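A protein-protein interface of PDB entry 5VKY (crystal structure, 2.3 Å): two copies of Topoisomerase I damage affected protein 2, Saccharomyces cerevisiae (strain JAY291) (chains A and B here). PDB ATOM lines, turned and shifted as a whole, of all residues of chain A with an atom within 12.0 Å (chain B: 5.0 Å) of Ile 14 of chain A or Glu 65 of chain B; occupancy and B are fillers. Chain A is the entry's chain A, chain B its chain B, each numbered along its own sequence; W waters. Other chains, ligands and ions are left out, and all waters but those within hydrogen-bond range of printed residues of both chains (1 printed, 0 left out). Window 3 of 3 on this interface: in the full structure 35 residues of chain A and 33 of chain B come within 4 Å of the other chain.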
ATOM      1  N   ILE A  14     -27.849   7.162 -19.056  1.00  0.00           N
ATOM      2  CA  ILE A  14     -26.747   6.885 -18.144  1.00  0.00           C
ATOM      3  C   ILE A  14     -26.040   8.167 -17.792  1.00  0.00           C
ATOM      4  O   ILE A  14     -25.631   8.919 -18.669  1.00  0.00           O
ATOM      5  CB  ILE A  14     -25.746   5.899 -18.733  1.00  0.00           C
ATOM      6  CG1 ILE A  14     -26.436   4.604 -19.140  1.00  0.00           C
ATOM      7  CG2 ILE A  14     -24.621   5.629 -17.742  1.00  0.00           C
ATOM      8  CD1 ILE A  14     -25.573   3.774 -19.994  1.00  0.00           C
ATOM      9  N   GLU A  15     -25.885   8.412 -16.498  1.00  0.00           N
ATOM     10  CA  GLU A  15     -25.250   9.626 -16.009  1.00  0.00           C
ATOM     11  C   GLU A  15     -24.235   9.239 -14.945  1.00  0.00           C
ATOM     12  O   GLU A  15     -24.589   8.594 -13.953  1.00  0.00           O
ATOM     13  CB  GLU A  15     -26.295  10.596 -15.446  1.00  0.00           C
ATOM     14  CG  GLU A  15     -25.732  11.917 -14.949  1.00  0.00           C
ATOM     15  CD  GLU A  15     -26.797  13.000 -14.816  1.00  0.00           C
ATOM     16  OE1 GLU A  15     -27.392  13.115 -13.721  1.00  0.00           O
ATOM     17  OE2 GLU A  15     -27.037  13.735 -15.807  1.00  0.00           O
ATOM     18  N   ILE A  16     -22.973   9.594 -15.173  1.00  0.00           N
ATOM     19  CA  ILE A  16     -21.961   9.535 -14.124  1.00  0.00           C
ATOM     20  C   ILE A  16     -22.217  10.685 -13.158  1.00  0.00           C
ATOM     21  O   ILE A  16     -22.290  11.852 -13.562  1.00  0.00           O
ATOM     22  CB  ILE A  16     -20.547   9.608 -14.719  1.00  0.00           C
ATOM     23  CG1 ILE A  16     -20.247   8.375 -15.584  1.00  0.00           C
ATOM     24  CG2 ILE A  16     -19.509   9.763 -13.620  1.00  0.00           C
ATOM     25  CD1 ILE A  16     -20.303   7.069 -14.829  1.00  0.00           C
ATOM     26  N   LYS A  17     -22.382  10.366 -11.879  1.00  0.00           N
ATOM     27  CA  LYS A  17     -22.739  11.393 -10.906  1.00  0.00           C
ATOM     28  C   LYS A  17     -21.514  12.207 -10.509  1.00  0.00           C
ATOM     29  O   LYS A  17     -20.447  11.654 -10.211  1.00  0.00           O
ATOM     30  CB  LYS A  17     -23.396  10.774  -9.676  1.00  0.00           C
ATOM     31  CG  LYS A  17     -24.828  10.279  -9.909  1.00  0.00           C
ATOM     32  CD  LYS A  17     -25.593  11.165 -10.892  1.00  0.00           C
ATOM     33  CE  LYS A  17     -26.542  12.122 -10.171  1.00  0.00           C
ATOM     34  NZ  LYS A  17     -27.423  12.861 -11.132  1.00  0.00           N
ATOM     35  N   ASP A  18     -21.685  13.527 -10.498  1.00  0.00           N
ATOM     36  CA  ASP A  18     -20.616  14.484 -10.242  1.00  0.00           C
ATOM     37  C   ASP A  18     -20.432  14.642  -8.737  1.00  0.00           C
ATOM     38  O   ASP A  18     -21.315  15.165  -8.047  1.00  0.00           O
ATOM     39  CB  ASP A  18     -20.957  15.822 -10.892  1.00  0.00           C
ATOM     40  CG  ASP A  18     -19.731  16.634 -11.250  1.00  0.00           C
ATOM     41  OD1 ASP A  18     -19.278  17.440 -10.409  1.00  0.00           O
ATOM     42  OD2 ASP A  18     -19.231  16.480 -12.383  1.00  0.00           O
ATOM     43  N   ASP A 100     -16.273   5.818  -8.008  1.00  0.00           N
ATOM     44  CA  ASP A 100     -17.091   6.435  -9.046  1.00  0.00           C
ATOM     45  C   ASP A 100     -18.492   5.849  -8.987  1.00  0.00           C
ATOM     46  O   ASP A 100     -18.672   4.682  -8.643  1.00  0.00           O
ATOM     47  CB  ASP A 100     -16.517   6.209 -10.439  1.00  0.00           C
ATOM     48  CG  ASP A 100     -15.083   6.618 -10.539  1.00  0.00           C
ATOM     49  OD1 ASP A 100     -14.829   7.834 -10.642  1.00  0.00           O
ATOM     50  OD2 ASP A 100     -14.210   5.725 -10.483  1.00  0.00           O
ATOM     51  N   ILE A 101     -19.480   6.647  -9.376  1.00  0.00           N
ATOM     52  CA  ILE A 101     -20.873   6.234  -9.282  1.00  0.00           C
ATOM     53  C   ILE A 101     -21.611   6.664 -10.537  1.00  0.00           C
ATOM     54  O   ILE A 101     -21.464   7.807 -10.985  1.00  0.00           O
ATOM     55  CB  ILE A 101     -21.575   6.834  -8.051  1.00  0.00           C
ATOM     56  CG1 ILE A 101     -21.027   6.213  -6.769  1.00  0.00           C
ATOM     57  CG2 ILE A 101     -23.066   6.552  -8.139  1.00  0.00           C
ATOM     58  CD1 ILE A 101     -21.998   6.257  -5.617  1.00  0.00           C
ATOM     59  N   GLY A 102     -22.421   5.759 -11.082  1.00  0.00           N
ATOM     60  CA  GLY A 102     -23.314   6.095 -12.170  1.00  0.00           C
ATOM     61  C   GLY A 102     -24.725   5.598 -11.906  1.00  0.00           C
ATOM     62  O   GLY A 102     -24.938   4.580 -11.243  1.00  0.00           O
ATOM     63  N   ALA A 103     -25.687   6.337 -12.457  1.00  0.00           N
ATOM     64  CA  ALA A 103     -27.105   6.012 -12.369  1.00  0.00           C
ATOM     65  C   ALA A 103     -27.686   5.809 -13.764  1.00  0.00           C
ATOM     66  O   ALA A 103     -27.245   6.432 -14.736  1.00  0.00           O
ATOM     67  CB  ALA A 103     -27.893   7.118 -11.648  1.00  0.00           C
ATOM     68  N   SER A 104     -28.701   4.944 -13.842  1.00  0.00           N
ATOM     69  CA  SER A 104     -29.392   4.619 -15.085  1.00  0.00           C
ATOM     70  C   SER A 104     -30.348   5.715 -15.554  1.00  0.00           C
ATOM     71  O   SER A 104     -30.990   5.545 -16.592  1.00  0.00           O
ATOM     72  CB  SER A 104     -30.165   3.305 -14.923  1.00  0.00           C
ATOM     73  OG  SER A 104     -31.234   3.455 -13.992  1.00  0.00           O
ATOM     74  N   TRP A 105     -30.466   6.825 -14.831  1.00  0.00           N
ATOM     75  CA  TRP A 105     -31.366   7.901 -15.220  1.00  0.00           C
ATOM     76  C   TRP A 105     -30.717   9.223 -14.855  1.00  0.00           C
ATOM     77  O   TRP A 105     -29.722   9.268 -14.132  1.00  0.00           O
ATOM     78  CB  TRP A 105     -32.737   7.770 -14.545  1.00  0.00           C
ATOM     79  CG  TRP A 105     -32.705   8.125 -13.091  1.00  0.00           C
ATOM     80  CD1 TRP A 105     -33.183   9.262 -12.515  1.00  0.00           C
ATOM     81  CD2 TRP A 105     -32.157   7.334 -12.025  1.00  0.00           C
ATOM     82  NE1 TRP A 105     -32.962   9.233 -11.157  1.00  0.00           N
ATOM     83  CE2 TRP A 105     -32.341   8.055 -10.832  1.00  0.00           C
ATOM     84  CE3 TRP A 105     -31.535   6.079 -11.966  1.00  0.00           C
ATOM     85  CZ2 TRP A 105     -31.921   7.570  -9.591  1.00  0.00           C
ATOM     86  CZ3 TRP A 105     -31.116   5.600 -10.731  1.00  0.00           C
ATOM     87  CH2 TRP A 105     -31.310   6.344  -9.565  1.00  0.00           C
ATOM     88  N   GLU A 106     -31.295  10.308 -15.361  1.00  0.00           N
ATOM     89  CA  GLU A 106     -30.787  11.652 -15.114  1.00  0.00           C
ATOM     90  C   GLU A 106     -31.800  12.453 -14.316  1.00  0.00           C
ATOM     91  O   GLU A 106     -32.924  12.680 -14.770  1.00  0.00           O
ATOM     92  CB  GLU A 106     -30.489  12.389 -16.411  1.00  0.00           C
ATOM     93  CG  GLU A 106     -29.995  11.524 -17.520  1.00  0.00           C
ATOM     94  CD  GLU A 106     -29.578  12.379 -18.663  1.00  0.00           C
ATOM     95  OE1 GLU A 106     -29.721  11.955 -19.835  1.00  0.00           O
ATOM     96  OE2 GLU A 106     -29.134  13.507 -18.354  1.00  0.00           O
ATOM     97  N   SER A 107     -31.390  12.896 -13.141  1.00  0.00           N
ATOM     98  CA  SER A 107     -32.116  13.894 -12.387  1.00  0.00           C
ATOM     99  C   SER A 107     -31.100  14.955 -12.026  1.00  0.00           C
ATOM    100  O   SER A 107     -30.025  14.633 -11.512  1.00  0.00           O
ATOM    101  CB  SER A 107     -32.769  13.296 -11.137  1.00  0.00           C
ATOM    102  OG  SER A 107     -33.333  14.305 -10.314  1.00  0.00           O
ATOM    103  N   LYS A 108     -31.400  16.202 -12.372  1.00  0.00           N
ATOM    104  CA  LYS A 108     -30.550  17.296 -11.935  1.00  0.00           C
ATOM    105  C   LYS A 108     -30.610  17.472 -10.425  1.00  0.00           C
ATOM    106  O   LYS A 108     -29.736  18.130  -9.852  1.00  0.00           O
ATOM    107  CB  LYS A 108     -30.943  18.595 -12.643  1.00  0.00           C
ATOM    108  CG  LYS A 108     -31.008  18.528 -14.199  1.00  0.00           C
ATOM    109  CD  LYS A 108     -32.353  18.037 -14.722  1.00  0.00           C
ATOM    110  CE  LYS A 108     -32.691  18.632 -16.086  1.00  0.00           C
ATOM    111  NZ  LYS A 108     -31.957  18.017 -17.229  1.00  0.00           N
ATOM    112  N   ASP A 110     -30.880  14.783  -8.103  1.00  0.00           N
ATOM    113  CA  ASP A 110     -30.105  13.735  -7.450  1.00  0.00           C
ATOM    114  C   ASP A 110     -28.621  14.077  -7.504  1.00  0.00           C
ATOM    115  O   ASP A 110     -28.144  14.678  -8.468  1.00  0.00           O
ATOM    116  CB  ASP A 110     -30.361  12.383  -8.119  1.00  0.00           C
ATOM    117  CG  ASP A 110     -31.836  12.046  -8.192  1.00  0.00           C
ATOM    118  OD1 ASP A 110     -32.628  12.746  -7.526  1.00  0.00           O
ATOM    119  OD2 ASP A 110     -32.209  11.105  -8.927  1.00  0.00           O
ATOM    120  N   LYS B  61     -20.359   2.287 -17.115  1.00  0.00           N
ATOM    121  CA  LYS B  61     -21.245   2.541 -18.251  1.00  0.00           C
ATOM    122  C   LYS B  61     -21.693   1.244 -18.908  1.00  0.00           C
ATOM    123  O   LYS B  61     -22.883   1.066 -19.195  1.00  0.00           O
ATOM    124  CB  LYS B  61     -20.545   3.431 -19.278  1.00  0.00           C
ATOM    125  CG  LYS B  61     -20.536   4.892 -18.901  1.00  0.00           C
ATOM    126  CD  LYS B  61     -19.332   5.616 -19.491  1.00  0.00           C
ATOM    127  CE  LYS B  61     -19.205   6.993 -18.891  1.00  0.00           C
ATOM    128  NZ  LYS B  61     -18.817   7.980 -19.914  1.00  0.00           N
ATOM    129  N   LEU B  62     -20.748   0.335 -19.165  1.00  0.00           N
ATOM    130  CA  LEU B  62     -21.096  -0.969 -19.721  1.00  0.00           C
ATOM    131  C   LEU B  62     -22.173  -1.643 -18.883  1.00  0.00           C
ATOM    132  O   LEU B  62     -23.223  -2.042 -19.400  1.00  0.00           O
ATOM    133  CB  LEU B  62     -19.846  -1.853 -19.804  1.00  0.00           C
ATOM    134  CG  LEU B  62     -18.978  -1.744 -21.055  1.00  0.00           C
ATOM    135  CD1 LEU B  62     -17.765  -2.675 -20.986  1.00  0.00           C
ATOM    136  CD2 LEU B  62     -19.803  -2.028 -22.312  1.00  0.00           C
ATOM    137  N   VAL B  63     -21.947  -1.730 -17.567  1.00  0.00           N
ATOM    138  CA  VAL B  63     -22.844  -2.501 -16.702  1.00  0.00           C
ATOM    139  C   VAL B  63     -24.245  -1.894 -16.695  1.00  0.00           C
ATOM    140  O   VAL B  63     -25.249  -2.621 -16.693  1.00  0.00           O
ATOM    141  CB  VAL B  63     -22.248  -2.600 -15.284  1.00  0.00           C
ATOM    142  CG1 VAL B  63     -23.283  -3.096 -14.281  1.00  0.00           C
ATOM    143  CG2 VAL B  63     -21.012  -3.507 -15.306  1.00  0.00           C
ATOM    144  N   LEU B  64     -24.337  -0.558 -16.716  1.00  0.00           N
ATOM    145  CA  LEU B  64     -25.641   0.099 -16.658  1.00  0.00           C
ATOM    146  C   LEU B  64     -26.407  -0.062 -17.974  1.00  0.00           C
ATOM    147  O   LEU B  64     -27.621  -0.308 -17.960  1.00  0.00           O
ATOM    148  CB  LEU B  64     -25.475   1.576 -16.284  1.00  0.00           C
ATOM    149  CG  LEU B  64     -25.003   1.847 -14.840  1.00  0.00           C
ATOM    150  CD1 LEU B  64     -24.643   3.292 -14.650  1.00  0.00           C
ATOM    151  CD2 LEU B  64     -26.040   1.429 -13.804  1.00  0.00           C
ATOM    152  N   GLU B  65     -25.720   0.073 -19.115  1.00  0.00           N
ATOM    153  CA  GLU B  65     -26.318  -0.253 -20.411  1.00  0.00           C
ATOM    154  C   GLU B  65     -26.980  -1.622 -20.372  1.00  0.00           C
ATOM    155  O   GLU B  65     -28.178  -1.769 -20.611  1.00  0.00           O
ATOM    156  CB  GLU B  65     -25.251  -0.236 -21.513  1.00  0.00           C
ATOM    157  CG  GLU B  65     -24.856   1.144 -21.994  1.00  0.00           C
ATOM    158  CD  GLU B  65     -23.528   1.144 -22.720  1.00  0.00           C
ATOM    159  OE1 GLU B  65     -23.210   0.121 -23.362  1.00  0.00           O
ATOM    160  OE2 GLU B  65     -22.812   2.166 -22.657  1.00  0.00           O
ATOM    161  N   LYS B  66     -26.207  -2.632 -20.023  1.00  0.00           N
ATOM    162  CA  LYS B  66     -26.684  -3.998 -20.115  1.00  0.00           C
ATOM    163  C   LYS B  66     -27.796  -4.290 -19.114  1.00  0.00           C
ATOM    164  O   LYS B  66     -28.691  -5.089 -19.403  1.00  0.00           O
ATOM    165  CB  LYS B  66     -25.506  -4.939 -19.923  1.00  0.00           C
ATOM    166  CG  LYS B  66     -24.372  -4.794 -20.960  1.00  0.00           C
ATOM    167  CD  LYS B  66     -23.286  -5.867 -20.760  1.00  0.00           C
ATOM    168  CE  LYS B  66     -22.096  -5.750 -21.716  1.00  0.00           C
ATOM    169  NZ  LYS B  66     -20.965  -6.572 -21.186  1.00  0.00           N
ATOM    170  N   LEU B  67     -27.750  -3.689 -17.921  1.00  0.00           N
ATOM    171  CA  LEU B  67     -28.862  -3.880 -16.995  1.00  0.00           C
ATOM    172  C   LEU B  67     -30.106  -3.159 -17.495  1.00  0.00           C
ATOM    173  O   LEU B  67     -31.230  -3.625 -17.276  1.00  0.00           O
ATOM    174  CB  LEU B  67     -28.487  -3.385 -15.599  1.00  0.00           C
ATOM    175  CG  LEU B  67     -27.619  -4.230 -14.658  1.00  0.00           C
ATOM    176  CD1 LEU B  67     -26.997  -3.286 -13.622  1.00  0.00           C
ATOM    177  CD2 LEU B  67     -28.400  -5.342 -13.955  1.00  0.00           C
ATOM    178  N   GLU B  68     -29.923  -2.005 -18.141  1.00  0.00           N
ATOM    179  CA  GLU B  68     -31.062  -1.267 -18.683  1.00  0.00           C
ATOM    180  C   GLU B  68     -31.759  -2.070 -19.767  1.00  0.00           C
ATOM    181  O   GLU B  68     -32.993  -2.056 -19.865  1.00  0.00           O
ATOM    182  CB  GLU B  68     -30.613   0.079 -19.248  1.00  0.00           C
ATOM    183  CG  GLU B  68     -30.638   1.236 -18.263  1.00  0.00           C
ATOM    184  CD  GLU B  68     -30.083   2.511 -18.876  1.00  0.00           C
ATOM    185  OE1 GLU B  68     -30.682   3.593 -18.668  1.00  0.00           O
ATOM    186  OE2 GLU B  68     -29.047   2.419 -19.578  1.00  0.00           O
ATOM    187  N   LYS B  69     -30.974  -2.770 -20.594  1.00  0.00           N
ATOM    188  CA  LYS B  69     -31.527  -3.586 -21.670  1.00  0.00           C
ATOM    189  C   LYS B  69     -32.361  -4.723 -21.118  1.00  0.00           C
ATOM    190  O   LYS B  69     -33.367  -5.111 -21.719  1.00  0.00           O
ATOM    191  CB  LYS B  69     -30.400  -4.156 -22.543  1.00  0.00           C
ATOM    192  CG  LYS B  69     -29.734  -3.149 -23.475  1.00  0.00           C
ATOM    193  CD  LYS B  69     -29.236  -3.820 -24.755  1.00  0.00           C
ATOM    194  CE  LYS B  69     -27.867  -3.300 -25.190  1.00  0.00           C
ATOM    195  NZ  LYS B  69     -27.201  -4.224 -26.161  1.00  0.00           N
HETATM  196  O   HOH W   1     -30.642   6.768 -20.013  1.00  0.00           O
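The backbone carbonyl oxygen of Glu 15 of chain A is in hydrogen-bond range of the backbone NH of Ala 103 of chain A (2.9 Å).
Among the printed residues, merely in contact across the chains: Ile 14 of chain A with Lys 61 of chain B, Ile 14 of chain A with Leu 64 of chain B, Ile 14 of chain A with Glu 65 of chain B, Ile 14 of chain A with Glu 68 of chain B, Ile 16 of chain A with Lys 61 of chain B, Gly 102 of chain A with Leu 64 of chain B and Ala 103 of chain A with Leu 64 of chain B.
Water W1 lies within hydrogen-bond range of N of Ile 14 of chain A (3.0 Å) and OE1 of Glu 68 of chain B (3.4 Å).
O of Ser 104 of chain A lies close to OE1 of Glu 68 of chain B (2.9 Å).
No position is printed for both chains.
Of the 8 pairs that touch across the chains among the printed residues, none has its exchanged pair printed and touching as well.
Hydrophobic or aromatic side chains of chain A that line the printed part of chain B: Ile 14 and Ile 16.
Printed residues of chain B that touch a printed residue of chain A: Lys 61, Leu 64, Glu 65 and Glu 68.
Hydrophobic or aromatic side chains of chain B that line the printed part of chain A: Leu 64.
Among the printed residues, no Asp or Glu carboxylate lies within 4 Å of a Lys or Arg side-chain nitrogen of the other chain.
Of the printed residues of chain B, Ile 16 of chain A touches Lys 61.
Printed residues of chain B within 4 Å of Gly 102 of chain A: Leu 64 (3.6 Å).
Printed residues of chain B within 4 Å of Ala 103 of chain A: Leu 64 (3.9 Å).
Printed residues of chain B within 4 Å of Ser 104 of chain A: Glu 68 (2.9 Å).
Trp 105 of chain A touches none of the printed residues of chain B.
Lys 61 of chain B touches just these residues of chain A: Ile 14 and Ile 16.
No residue of chain A comes within 4 Å of Val 63 of chain B.
Of the printed residues of chain A, Leu 64 of chain B touches Ile 14, Gly 102 and Ala 103.
Glu 65 of chain B touches one residue of chain A.
Of chain A, only Ile 14 and Ser 104 come within 4 Å of Glu 68 of chain B.
No residue of chain A comes within 4 Å of Lys 69 of chain B.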
